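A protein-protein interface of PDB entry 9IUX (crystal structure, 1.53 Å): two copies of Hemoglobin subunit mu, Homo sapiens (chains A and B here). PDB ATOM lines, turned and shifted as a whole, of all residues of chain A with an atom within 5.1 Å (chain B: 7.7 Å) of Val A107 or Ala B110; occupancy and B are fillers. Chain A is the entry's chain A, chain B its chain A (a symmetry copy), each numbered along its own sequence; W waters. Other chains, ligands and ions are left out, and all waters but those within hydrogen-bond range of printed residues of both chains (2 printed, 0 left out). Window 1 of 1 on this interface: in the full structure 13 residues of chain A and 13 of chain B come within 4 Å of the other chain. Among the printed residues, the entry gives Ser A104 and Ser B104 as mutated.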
ATOM      1  N   ARG A  31       9.764  20.957  31.582  1.00  0.00           N
ATOM      2  CA  ARG A  31      10.413  19.651  31.607  1.00  0.00           C
ATOM      3  C   ARG A  31      11.606  19.678  32.544  1.00  0.00           C
ATOM      4  O   ARG A  31      11.785  18.764  33.359  1.00  0.00           O
ATOM      5  CB  ARG A  31      10.814  19.259  30.182  1.00  0.00           C
ATOM      6  CG  ARG A  31      11.156  17.793  29.994  1.00  0.00           C
ATOM      7  CD  ARG A  31      12.639  17.549  29.979  1.00  0.00           C
ATOM      8  NE  ARG A  31      12.903  16.123  29.798  1.00  0.00           N
ATOM      9  CZ  ARG A  31      14.044  15.526  30.111  1.00  0.00           C
ATOM     10  NH1 ARG A  31      15.090  16.215  30.550  1.00  0.00           N
ATOM     11  NH2 ARG A  31      14.137  14.202  29.984  1.00  0.00           N
ATOM     12  N   GLN A 103      19.971  18.837  27.540  1.00  0.00           N
ATOM     13  CA  GLN A 103      19.284  17.552  27.359  1.00  0.00           C
ATOM     14  C   GLN A 103      17.773  17.726  27.295  1.00  0.00           C
ATOM     15  O   GLN A 103      17.092  17.059  26.498  1.00  0.00           O
ATOM     16  CB  GLN A 103      19.656  16.585  28.481  1.00  0.00           C
ATOM     17  CG  GLN A 103      21.153  16.327  28.595  1.00  0.00           C
ATOM     18  CD  GLN A 103      21.588  16.021  30.023  1.00  0.00           C
ATOM     19  OE1 GLN A 103      20.764  15.726  30.892  1.00  0.00           O
ATOM     20  NE2 GLN A 103      22.888  16.098  30.271  1.00  0.00           N
ATOM     21  N   SER A 104      17.230  18.583  28.156  1.00  0.00           N
ATOM     22  CA  SER A 104      15.795  18.835  28.163  1.00  0.00           C
ATOM     23  C   SER A 104      15.353  19.458  26.849  1.00  0.00           C
ATOM     24  O   SER A 104      14.267  19.158  26.335  1.00  0.00           O
ATOM     25  CB  SER A 104      15.437  19.742  29.350  1.00  0.00           C
ATOM     26  OG  SER A 104      15.703  19.098  30.592  1.00  0.00           O
ATOM     27  N   PHE A 105      16.197  20.315  26.274  1.00  0.00           N
ATOM     28  CA  PHE A 105      15.860  20.984  25.022  1.00  0.00           C
ATOM     29  C   PHE A 105      15.758  19.980  23.874  1.00  0.00           C
ATOM     30  O   PHE A 105      14.823  20.053  23.066  1.00  0.00           O
ATOM     31  CB  PHE A 105      16.917  22.065  24.768  1.00  0.00           C
ATOM     32  CG  PHE A 105      16.545  23.108  23.749  1.00  0.00           C
ATOM     33  CD1 PHE A 105      15.287  23.166  23.174  1.00  0.00           C
ATOM     34  CD2 PHE A 105      17.463  24.095  23.439  1.00  0.00           C
ATOM     35  CE1 PHE A 105      14.981  24.158  22.239  1.00  0.00           C
ATOM     36  CE2 PHE A 105      17.166  25.088  22.517  1.00  0.00           C
ATOM     37  CZ  PHE A 105      15.931  25.117  21.916  1.00  0.00           C
ATOM     38  N   HIS A 106      16.682  19.014  23.810  1.00  0.00           N
ATOM     39  CA  HIS A 106      16.579  17.960  22.796  1.00  0.00           C
ATOM     40  C   HIS A 106      15.256  17.213  22.889  1.00  0.00           C
ATOM     41  O   HIS A 106      14.663  16.862  21.861  1.00  0.00           O
ATOM     42  CB  HIS A 106      17.714  16.934  22.921  1.00  0.00           C
ATOM     43  CG  HIS A 106      19.078  17.478  22.635  1.00  0.00           C
ATOM     44  ND1 HIS A 106      19.371  18.200  21.500  1.00  0.00           N
ATOM     45  CD2 HIS A 106      20.238  17.381  23.328  1.00  0.00           C
ATOM     46  CE1 HIS A 106      20.652  18.533  21.509  1.00  0.00           C
ATOM     47  NE2 HIS A 106      21.196  18.064  22.619  1.00  0.00           N
ATOM     48  N   VAL A 107      14.796  16.926  24.117  1.00  0.00           N
ATOM     49  CA  VAL A 107      13.559  16.161  24.291  1.00  0.00           C
ATOM     50  C   VAL A 107      12.370  16.963  23.793  1.00  0.00           C
ATOM     51  O   VAL A 107      11.499  16.439  23.098  1.00  0.00           O
ATOM     52  CB  VAL A 107      13.376  15.751  25.764  1.00  0.00           C
ATOM     53  CG1 VAL A 107      12.008  15.067  25.955  1.00  0.00           C
ATOM     54  CG2 VAL A 107      14.501  14.827  26.216  1.00  0.00           C
ATOM     55  N   VAL A 108      12.314  18.250  24.140  1.00  0.00           N
ATOM     56  CA  VAL A 108      11.202  19.081  23.681  1.00  0.00           C
ATOM     57  C   VAL A 108      11.196  19.175  22.159  1.00  0.00           C
ATOM     58  O   VAL A 108      10.149  19.050  21.513  1.00  0.00           O
ATOM     59  CB  VAL A 108      11.283  20.470  24.348  1.00  0.00           C
ATOM     60  CG1 VAL A 108      10.320  21.450  23.700  1.00  0.00           C
ATOM     61  CG2 VAL A 108      11.026  20.350  25.853  1.00  0.00           C
ATOM     62  N   LEU A 109      12.366  19.396  21.555  1.00  0.00           N
ATOM     63  CA  LEU A 109      12.425  19.462  20.096  1.00  0.00           C
ATOM     64  C   LEU A 109      11.986  18.145  19.456  1.00  0.00           C
ATOM     65  O   LEU A 109      11.247  18.143  18.473  1.00  0.00           O
ATOM     66  CB  LEU A 109      13.837  19.826  19.649  1.00  0.00           C
ATOM     67  CG  LEU A 109      14.246  21.273  19.949  1.00  0.00           C
ATOM     68  CD1 LEU A 109      15.715  21.498  19.617  1.00  0.00           C
ATOM     69  CD2 LEU A 109      13.379  22.261  19.192  1.00  0.00           C
ATOM     70  N   ALA A 110      12.424  17.013  20.006  1.00  0.00           N
ATOM     71  CA  ALA A 110      12.027  15.722  19.456  1.00  0.00           C
ATOM     72  C   ALA A 110      10.521  15.517  19.541  1.00  0.00           C
ATOM     73  O   ALA A 110       9.906  14.975  18.615  1.00  0.00           O
ATOM     74  CB  ALA A 110      12.757  14.602  20.205  1.00  0.00           C
ATOM     75  N   SER A 111       9.909  15.938  20.650  1.00  0.00           N
ATOM     76  CA  SER A 111       8.473  15.753  20.819  1.00  0.00           C
ATOM     77  C   SER A 111       7.682  16.493  19.753  1.00  0.00           C
ATOM     78  O   SER A 111       6.634  16.009  19.316  1.00  0.00           O
ATOM     79  CB  SER A 111       8.048  16.225  22.209  1.00  0.00           C
ATOM     80  OG  SER A 111       6.668  15.976  22.423  1.00  0.00           O
ATOM     81  N   ARG B  31      21.182   7.060  17.668  1.00  0.00           N
ATOM     82  CA  ARG B  31      21.284   8.407  18.219  1.00  0.00           C
ATOM     83  C   ARG B  31      22.496   8.511  19.124  1.00  0.00           C
ATOM     84  O   ARG B  31      23.266   9.477  19.036  1.00  0.00           O
ATOM     85  CB  ARG B  31      19.986   8.750  18.957  1.00  0.00           C
ATOM     86  CG  ARG B  31      19.794  10.224  19.259  1.00  0.00           C
ATOM     87  CD  ARG B  31      20.144  10.567  20.679  1.00  0.00           C
ATOM     88  NE  ARG B  31      19.941  11.997  20.906  1.00  0.00           N
ATOM     89  CZ  ARG B  31      20.496  12.686  21.893  1.00  0.00           C
ATOM     90  NH1 ARG B  31      21.235  12.094  22.822  1.00  0.00           N
ATOM     91  NH2 ARG B  31      20.307  14.005  21.946  1.00  0.00           N
ATOM     92  N   ILE B 102      20.744   6.982  28.656  1.00  0.00           N
ATOM     93  CA  ILE B 102      19.456   7.359  29.241  1.00  0.00           C
ATOM     94  C   ILE B 102      18.924   8.635  28.590  1.00  0.00           C
ATOM     95  O   ILE B 102      17.761   8.692  28.171  1.00  0.00           O
ATOM     96  CB  ILE B 102      19.584   7.495  30.772  1.00  0.00           C
ATOM     97  CG1 ILE B 102      19.900   6.133  31.394  1.00  0.00           C
ATOM     98  CG2 ILE B 102      18.319   8.108  31.389  1.00  0.00           C
ATOM     99  CD1 ILE B 102      20.301   6.223  32.861  1.00  0.00           C
ATOM    100  N   GLN B 103      19.772   9.658  28.451  1.00  0.00           N
ATOM    101  CA  GLN B 103      19.332  10.882  27.769  1.00  0.00           C
ATOM    102  C   GLN B 103      18.893  10.602  26.338  1.00  0.00           C
ATOM    103  O   GLN B 103      17.904  11.178  25.855  1.00  0.00           O
ATOM    104  CB  GLN B 103      20.444  11.929  27.784  1.00  0.00           C
ATOM    105  CG  GLN B 103      20.922  12.295  29.183  1.00  0.00           C
ATOM    106  CD  GLN B 103      22.389  12.704  29.213  1.00  0.00           C
ATOM    107  OE1 GLN B 103      22.994  12.987  28.176  1.00  0.00           O
ATOM    108  NE2 GLN B 103      22.968  12.730  30.405  1.00  0.00           N
ATOM    109  N   SER B 104      19.641   9.756  25.635  1.00  0.00           N
ATOM    110  CA  SER B 104      19.295   9.408  24.263  1.00  0.00           C
ATOM    111  C   SER B 104      17.958   8.687  24.214  1.00  0.00           C
ATOM    112  O   SER B 104      17.162   8.885  23.286  1.00  0.00           O
ATOM    113  CB  SER B 104      20.410   8.541  23.656  1.00  0.00           C
ATOM    114  OG  SER B 104      21.631   9.266  23.553  1.00  0.00           O
ATOM    115  N   PHE B 105      17.680   7.861  25.222  1.00  0.00           N
ATOM    116  CA  PHE B 105      16.432   7.106  25.259  1.00  0.00           C
ATOM    117  C   PHE B 105      15.231   8.039  25.408  1.00  0.00           C
ATOM    118  O   PHE B 105      14.216   7.860  24.723  1.00  0.00           O
ATOM    119  CB  PHE B 105      16.534   6.088  26.401  1.00  0.00           C
ATOM    120  CG  PHE B 105      15.527   4.970  26.364  1.00  0.00           C
ATOM    121  CD1 PHE B 105      14.653   4.796  25.305  1.00  0.00           C
ATOM    122  CD2 PHE B 105      15.532   4.033  27.381  1.00  0.00           C
ATOM    123  CE1 PHE B 105      13.740   3.738  25.306  1.00  0.00           C
ATOM    124  CE2 PHE B 105      14.635   2.975  27.389  1.00  0.00           C
ATOM    125  CZ  PHE B 105      13.739   2.831  26.357  1.00  0.00           C
ATOM    126  N   HIS B 106      15.341   9.062  26.266  1.00  0.00           N
ATOM    127  CA  HIS B 106      14.265  10.051  26.376  1.00  0.00           C
ATOM    128  C   HIS B 106      13.963  10.710  25.038  1.00  0.00           C
ATOM    129  O   HIS B 106      12.795  10.966  24.717  1.00  0.00           O
ATOM    130  CB  HIS B 106      14.608  11.158  27.384  1.00  0.00           C
ATOM    131  CG  HIS B 106      14.721  10.694  28.802  1.00  0.00           C
ATOM    132  ND1 HIS B 106      13.752   9.935  29.418  1.00  0.00           N
ATOM    133  CD2 HIS B 106      15.682  10.906  29.734  1.00  0.00           C
ATOM    134  CE1 HIS B 106      14.114   9.692  30.669  1.00  0.00           C
ATOM    135  NE2 HIS B 106      15.292  10.254  30.878  1.00  0.00           N
ATOM    136  N   VAL B 107      15.008  11.029  24.258  1.00  0.00           N
ATOM    137  CA  VAL B 107      14.805  11.715  22.981  1.00  0.00           C
ATOM    138  C   VAL B 107      14.073  10.809  22.007  1.00  0.00           C
ATOM    139  O   VAL B 107      13.143  11.235  21.322  1.00  0.00           O
ATOM    140  CB  VAL B 107      16.150  12.189  22.398  1.00  0.00           C
ATOM    141  CG1 VAL B 107      15.934  12.787  20.994  1.00  0.00           C
ATOM    142  CG2 VAL B 107      16.812  13.210  23.315  1.00  0.00           C
ATOM    143  N   VAL B 108      14.481   9.541  21.930  1.00  0.00           N
ATOM    144  CA  VAL B 108      13.809   8.614  21.021  1.00  0.00           C
ATOM    145  C   VAL B 108      12.347   8.440  21.419  1.00  0.00           C
ATOM    146  O   VAL B 108      11.446   8.459  20.572  1.00  0.00           O
ATOM    147  CB  VAL B 108      14.567   7.270  20.998  1.00  0.00           C
ATOM    148  CG1 VAL B 108      13.762   6.194  20.290  1.00  0.00           C
ATOM    149  CG2 VAL B 108      15.943   7.451  20.350  1.00  0.00           C
ATOM    150  N   LEU B 109      12.081   8.268  22.715  1.00  0.00           N
ATOM    151  CA  LEU B 109      10.695   8.130  23.157  1.00  0.00           C
ATOM    152  C   LEU B 109       9.876   9.379  22.833  1.00  0.00           C
ATOM    153  O   LEU B 109       8.737   9.278  22.377  1.00  0.00           O
ATOM    154  CB  LEU B 109      10.654   7.840  24.654  1.00  0.00           C
ATOM    155  CG  LEU B 109      11.146   6.442  25.046  1.00  0.00           C
ATOM    156  CD1 LEU B 109      11.221   6.301  26.560  1.00  0.00           C
ATOM    157  CD2 LEU B 109      10.261   5.359  24.460  1.00  0.00           C
ATOM    158  N   ALA B 110      10.441  10.564  23.052  1.00  0.00           N
ATOM    159  CA  ALA B 110       9.720  11.795  22.745  1.00  0.00           C
ATOM    160  C   ALA B 110       9.400  11.900  21.261  1.00  0.00           C
ATOM    161  O   ALA B 110       8.312  12.350  20.882  1.00  0.00           O
ATOM    162  CB  ALA B 110      10.553  12.999  23.195  1.00  0.00           C
ATOM    163  N   SER B 111      10.340  11.498  20.403  1.00  0.00           N
ATOM    164  CA  SER B 111      10.120  11.592  18.965  1.00  0.00           C
ATOM    165  C   SER B 111       8.939  10.745  18.520  1.00  0.00           C
ATOM    166  O   SER B 111       8.215  11.133  17.599  1.00  0.00           O
ATOM    167  CB  SER B 111      11.382  11.166  18.217  1.00  0.00           C
ATOM    168  OG  SER B 111      11.216  11.331  16.818  1.00  0.00           O
ATOM    169  N   HIS B 112       8.727   9.595  19.160  1.00  0.00           N
ATOM    170  CA  HIS B 112       7.657   8.686  18.761  1.00  0.00           C
ATOM    171  C   HIS B 112       6.365   8.953  19.509  1.00  0.00           C
ATOM    172  O   HIS B 112       5.278   8.873  18.922  1.00  0.00           O
ATOM    173  CB  HIS B 112       8.092   7.238  18.994  1.00  0.00           C
ATOM    174  CG  HIS B 112       9.079   6.747  17.986  1.00  0.00           C
ATOM    175  ND1 HIS B 112       8.703   6.284  16.743  1.00  0.00           N
ATOM    176  CD2 HIS B 112      10.429   6.677  18.023  1.00  0.00           C
ATOM    177  CE1 HIS B 112       9.782   5.935  16.063  1.00  0.00           C
ATOM    178  NE2 HIS B 112      10.842   6.161  16.817  1.00  0.00           N
ATOM    179  N   LEU B 113       6.463   9.276  20.791  1.00  0.00           N
ATOM    180  CA  LEU B 113       5.284   9.370  21.635  1.00  0.00           C
ATOM    181  C   LEU B 113       4.768  10.789  21.770  1.00  0.00           C
ATOM    182  O   LEU B 113       3.606  10.969  22.146  1.00  0.00           O
ATOM    183  CB  LEU B 113       5.583   8.810  23.024  1.00  0.00           C
ATOM    184  CG  LEU B 113       6.057   7.358  23.053  1.00  0.00           C
ATOM    185  CD1 LEU B 113       6.258   6.922  24.499  1.00  0.00           C
ATOM    186  CD2 LEU B 113       5.054   6.459  22.318  1.00  0.00           C
ATOM    187  N   GLN B 114       5.600  11.787  21.463  1.00  0.00           N
ATOM    188  CA  GLN B 114       5.264  13.218  21.529  1.00  0.00           C
ATOM    189  C   GLN B 114       4.693  13.526  22.912  1.00  0.00           C
ATOM    190  O   GLN B 114       5.276  13.115  23.926  1.00  0.00           O
ATOM    191  CB  GLN B 114       4.359  13.588  20.374  1.00  0.00           C
ATOM    192  CG  GLN B 114       4.915  13.208  19.029  1.00  0.00           C
ATOM    193  CD  GLN B 114       4.136  13.862  17.921  1.00  0.00           C
ATOM    194  OE1 GLN B 114       3.120  13.331  17.469  1.00  0.00           O
ATOM    195  NE2 GLN B 114       4.583  15.046  17.499  1.00  0.00           N
ATOM    196  N   ASP B 115       3.567  14.228  23.007  1.00  0.00           N
ATOM    197  CA  ASP B 115       3.079  14.664  24.305  1.00  0.00           C
ATOM    198  C   ASP B 115       2.487  13.540  25.146  1.00  0.00           C
ATOM    199  O   ASP B 115       2.198  13.771  26.325  1.00  0.00           O
ATOM    200  CB  ASP B 115       2.067  15.798  24.103  1.00  0.00           C
ATOM    201  CG  ASP B 115       0.920  15.399  23.199  1.00  0.00           C
ATOM    202  OD1 ASP B 115      -0.245  15.602  23.598  1.00  0.00           O
ATOM    203  OD2 ASP B 115       1.183  14.902  22.078  1.00  0.00           O
ATOM    204  N   GLU B 116       2.331  12.332  24.598  1.00  0.00           N
ATOM    205  CA  GLU B 116       1.958  11.196  25.435  1.00  0.00           C
ATOM    206  C   GLU B 116       3.052  10.846  26.429  1.00  0.00           C
ATOM    207  O   GLU B 116       2.770  10.237  27.463  1.00  0.00           O
ATOM    208  CB  GLU B 116       1.633   9.977  24.562  1.00  0.00           C
ATOM    209  CG  GLU B 116       0.406  10.158  23.666  1.00  0.00           C
ATOM    210  CD  GLU B 116      -0.857  10.546  24.439  1.00  0.00           C
ATOM    211  OE1 GLU B 116      -1.031  10.085  25.590  1.00  0.00           O
ATOM    212  OE2 GLU B 116      -1.683  11.312  23.894  1.00  0.00           O
ATOM    213  N   PHE B 117       4.300  11.206  26.130  1.00  0.00           N
ATOM    214  CA  PHE B 117       5.433  10.986  27.031  1.00  0.00           C
ATOM    215  C   PHE B 117       5.538  12.247  27.891  1.00  0.00           C
ATOM    216  O   PHE B 117       6.305  13.175  27.615  1.00  0.00           O
ATOM    217  CB  PHE B 117       6.686  10.707  26.201  1.00  0.00           C
ATOM    218  CG  PHE B 117       7.911  10.272  26.979  1.00  0.00           C
ATOM    219  CD1 PHE B 117       7.841   9.360  28.008  1.00  0.00           C
ATOM    220  CD2 PHE B 117       9.154  10.772  26.615  1.00  0.00           C
ATOM    221  CE1 PHE B 117       8.996   8.961  28.680  1.00  0.00           C
ATOM    222  CE2 PHE B 117      10.316  10.368  27.271  1.00  0.00           C
ATOM    223  CZ  PHE B 117      10.225   9.468  28.308  1.00  0.00           C
ATOM    224  N   THR B 118       4.709  12.296  28.935  1.00  0.00           N
ATOM    225  CA  THR B 118       4.549  13.528  29.699  1.00  0.00           C
ATOM    226  C   THR B 118       5.767  13.800  30.568  1.00  0.00           C
ATOM    227  O   THR B 118       6.596  12.921  30.810  1.00  0.00           O
ATOM    228  CB  THR B 118       3.333  13.453  30.608  1.00  0.00           C
ATOM    229  OG1 THR B 118       3.600  12.511  31.659  1.00  0.00           O
ATOM    230  CG2 THR B 118       2.091  13.061  29.840  1.00  0.00           C
ATOM    231  N   VAL B 119       5.860  15.035  31.079  1.00  0.00           N
ATOM    232  CA  VAL B 119       7.027  15.336  31.904  1.00  0.00           C
ATOM    233  C   VAL B 119       6.998  14.525  33.196  1.00  0.00           C
ATOM    234  O   VAL B 119       8.052  14.129  33.708  1.00  0.00           O
ATOM    235  CB  VAL B 119       7.159  16.855  32.168  1.00  0.00           C
ATOM    236  CG1 VAL B 119       7.467  17.580  30.866  1.00  0.00           C
ATOM    237  CG2 VAL B 119       5.929  17.431  32.855  1.00  0.00           C
ATOM    238  N   GLN B 122       8.384  11.222  32.238  1.00  0.00           N
ATOM    239  CA  GLN B 122       9.833  11.303  32.028  1.00  0.00           C
ATOM    240  C   GLN B 122      10.593  11.330  33.347  1.00  0.00           C
ATOM    241  O   GLN B 122      11.655  10.710  33.469  1.00  0.00           O
ATOM    242  CB  GLN B 122      10.166  12.557  31.231  1.00  0.00           C
ATOM    243  CG  GLN B 122       9.622  12.534  29.825  1.00  0.00           C
ATOM    244  CD  GLN B 122       9.984  13.786  29.099  1.00  0.00           C
ATOM    245  OE1 GLN B 122      11.124  14.246  29.173  1.00  0.00           O
ATOM    246  NE2 GLN B 122       9.012  14.375  28.412  1.00  0.00           N
HETATM  247  O   HOH W   1       7.556  13.945  25.075  1.00  0.00           O
HETATM  248  O   HOH W   2      18.101  14.151  26.639  1.00  0.00           O
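Water W1 lies within hydrogen-bond range of the backbone carbonyl oxygen (O) of Gln B114 (2.7 Å), the backbone carbonyl oxygen (O) of Phe B117 (2.9 Å) and the side-chain hydroxyl (OG) of Ser A111 (3.5 Å).
Water W2 bridges the backbone carbonyl oxygen (O) of Gln A103 (3.1 Å) and the backbone carbonyl oxygen (O) of Gln B103 (3.1 Å).
His A106 touches Val B107, and with the chains exchanged Val A107 touches His B106.
Val A107 touches Ala B110, and with the chains exchanged Ala A110 touches Val B107.
Ala B110 touches its own counterpart, Ala A110.
Ala A110 touches Ser B111, and with the chains exchanged Ser A111 touches Ala B110.
Positions printed for both chains: 31, 103, 104, 105, 106, 107, 108, 109, 110 and 111.
Of the 15 pairs that touch across the chains among the printed residues, 10 have their exchanged pair printed and touching as well.
Printed residues of chain A that touch a printed residue of chain B: Arg A31, Gln A103, His A106, Val A107, Ala A110 and Ser A111.
Along chain B the printed residues that touch a printed residue of chain A span positions 31 to 122.
Among the printed residues, 15 pairs touch across the chains.
Of the printed residues of chain B, Gln A103 touches Gln B103 (3.4 Å).
Of chain B, only His B106, Ala B110 and Gln B122 come within 4 Å of Val A107.
Of the printed residues of chain B, Ala A110 touches Val B107 (3.6 Å), Ala B110 (3.8 Å) and Ser B111 (3.4 Å).
Of the printed residues of chain A, Arg B31 touches His A106 (3.6 Å).
Printed residues of chain A within 4 Å of Val B107: His A106 and Ala A110.
Val B108 touches none of the printed residues of chain A.
Of the printed residues of chain A, Ala B110 touches Val A107, Ala A110 and Ser A111.
Printed residues of chain A within 4 Å of Gln B114: Ser A111 (2.9 Å).
The nearest residue of chain B that does not touch Val A107 is Val B107 (4.05 Å).
NE of Arg A31 is in hydrogen-bond range of OE1 of Gln B122 (2.7 Å).
O of Ser A111 is in hydrogen-bond range of NE2 of Gln B114, 2.9 Å away.
The side-chain amide nitrogen (NE2) of Gln A103 sits close to the side-chain amide nitrogen (NE2) of Gln B103 (3.4 Å).
NH2 of Arg A31 touches CD2 of His B106 (3.6 Å).
CA of Arg A31 touches CG1 of Val B119 (3.7 Å).
Arg B31 touches His A106.
His A106 touches Val B107 (CB to CG2, 3.9 Å).
Val A107 touches Ala B110.
Val A107 touches Gln B122 (CG1 to OE1, 3.4 Å).
Ala A110 touches Ala B110.
Ser B111 touches Ala A110 (CA to O, 3.4 Å).
Ser A111 touches Ala B110.
Asp B115 touches Ser A111.
NE2 of Gln B122 is in hydrogen-bond range of O of Phe B117, 3.1 Å away.
The guanidinium group (NH1) of Arg A31 lies within hydrogen-bond range of the side-chain hydroxyl (OG) of Ser A104 (2.9 Å).
NH1 of Arg B31 is in hydrogen-bond range of OG of Ser B104 (2.9 Å).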
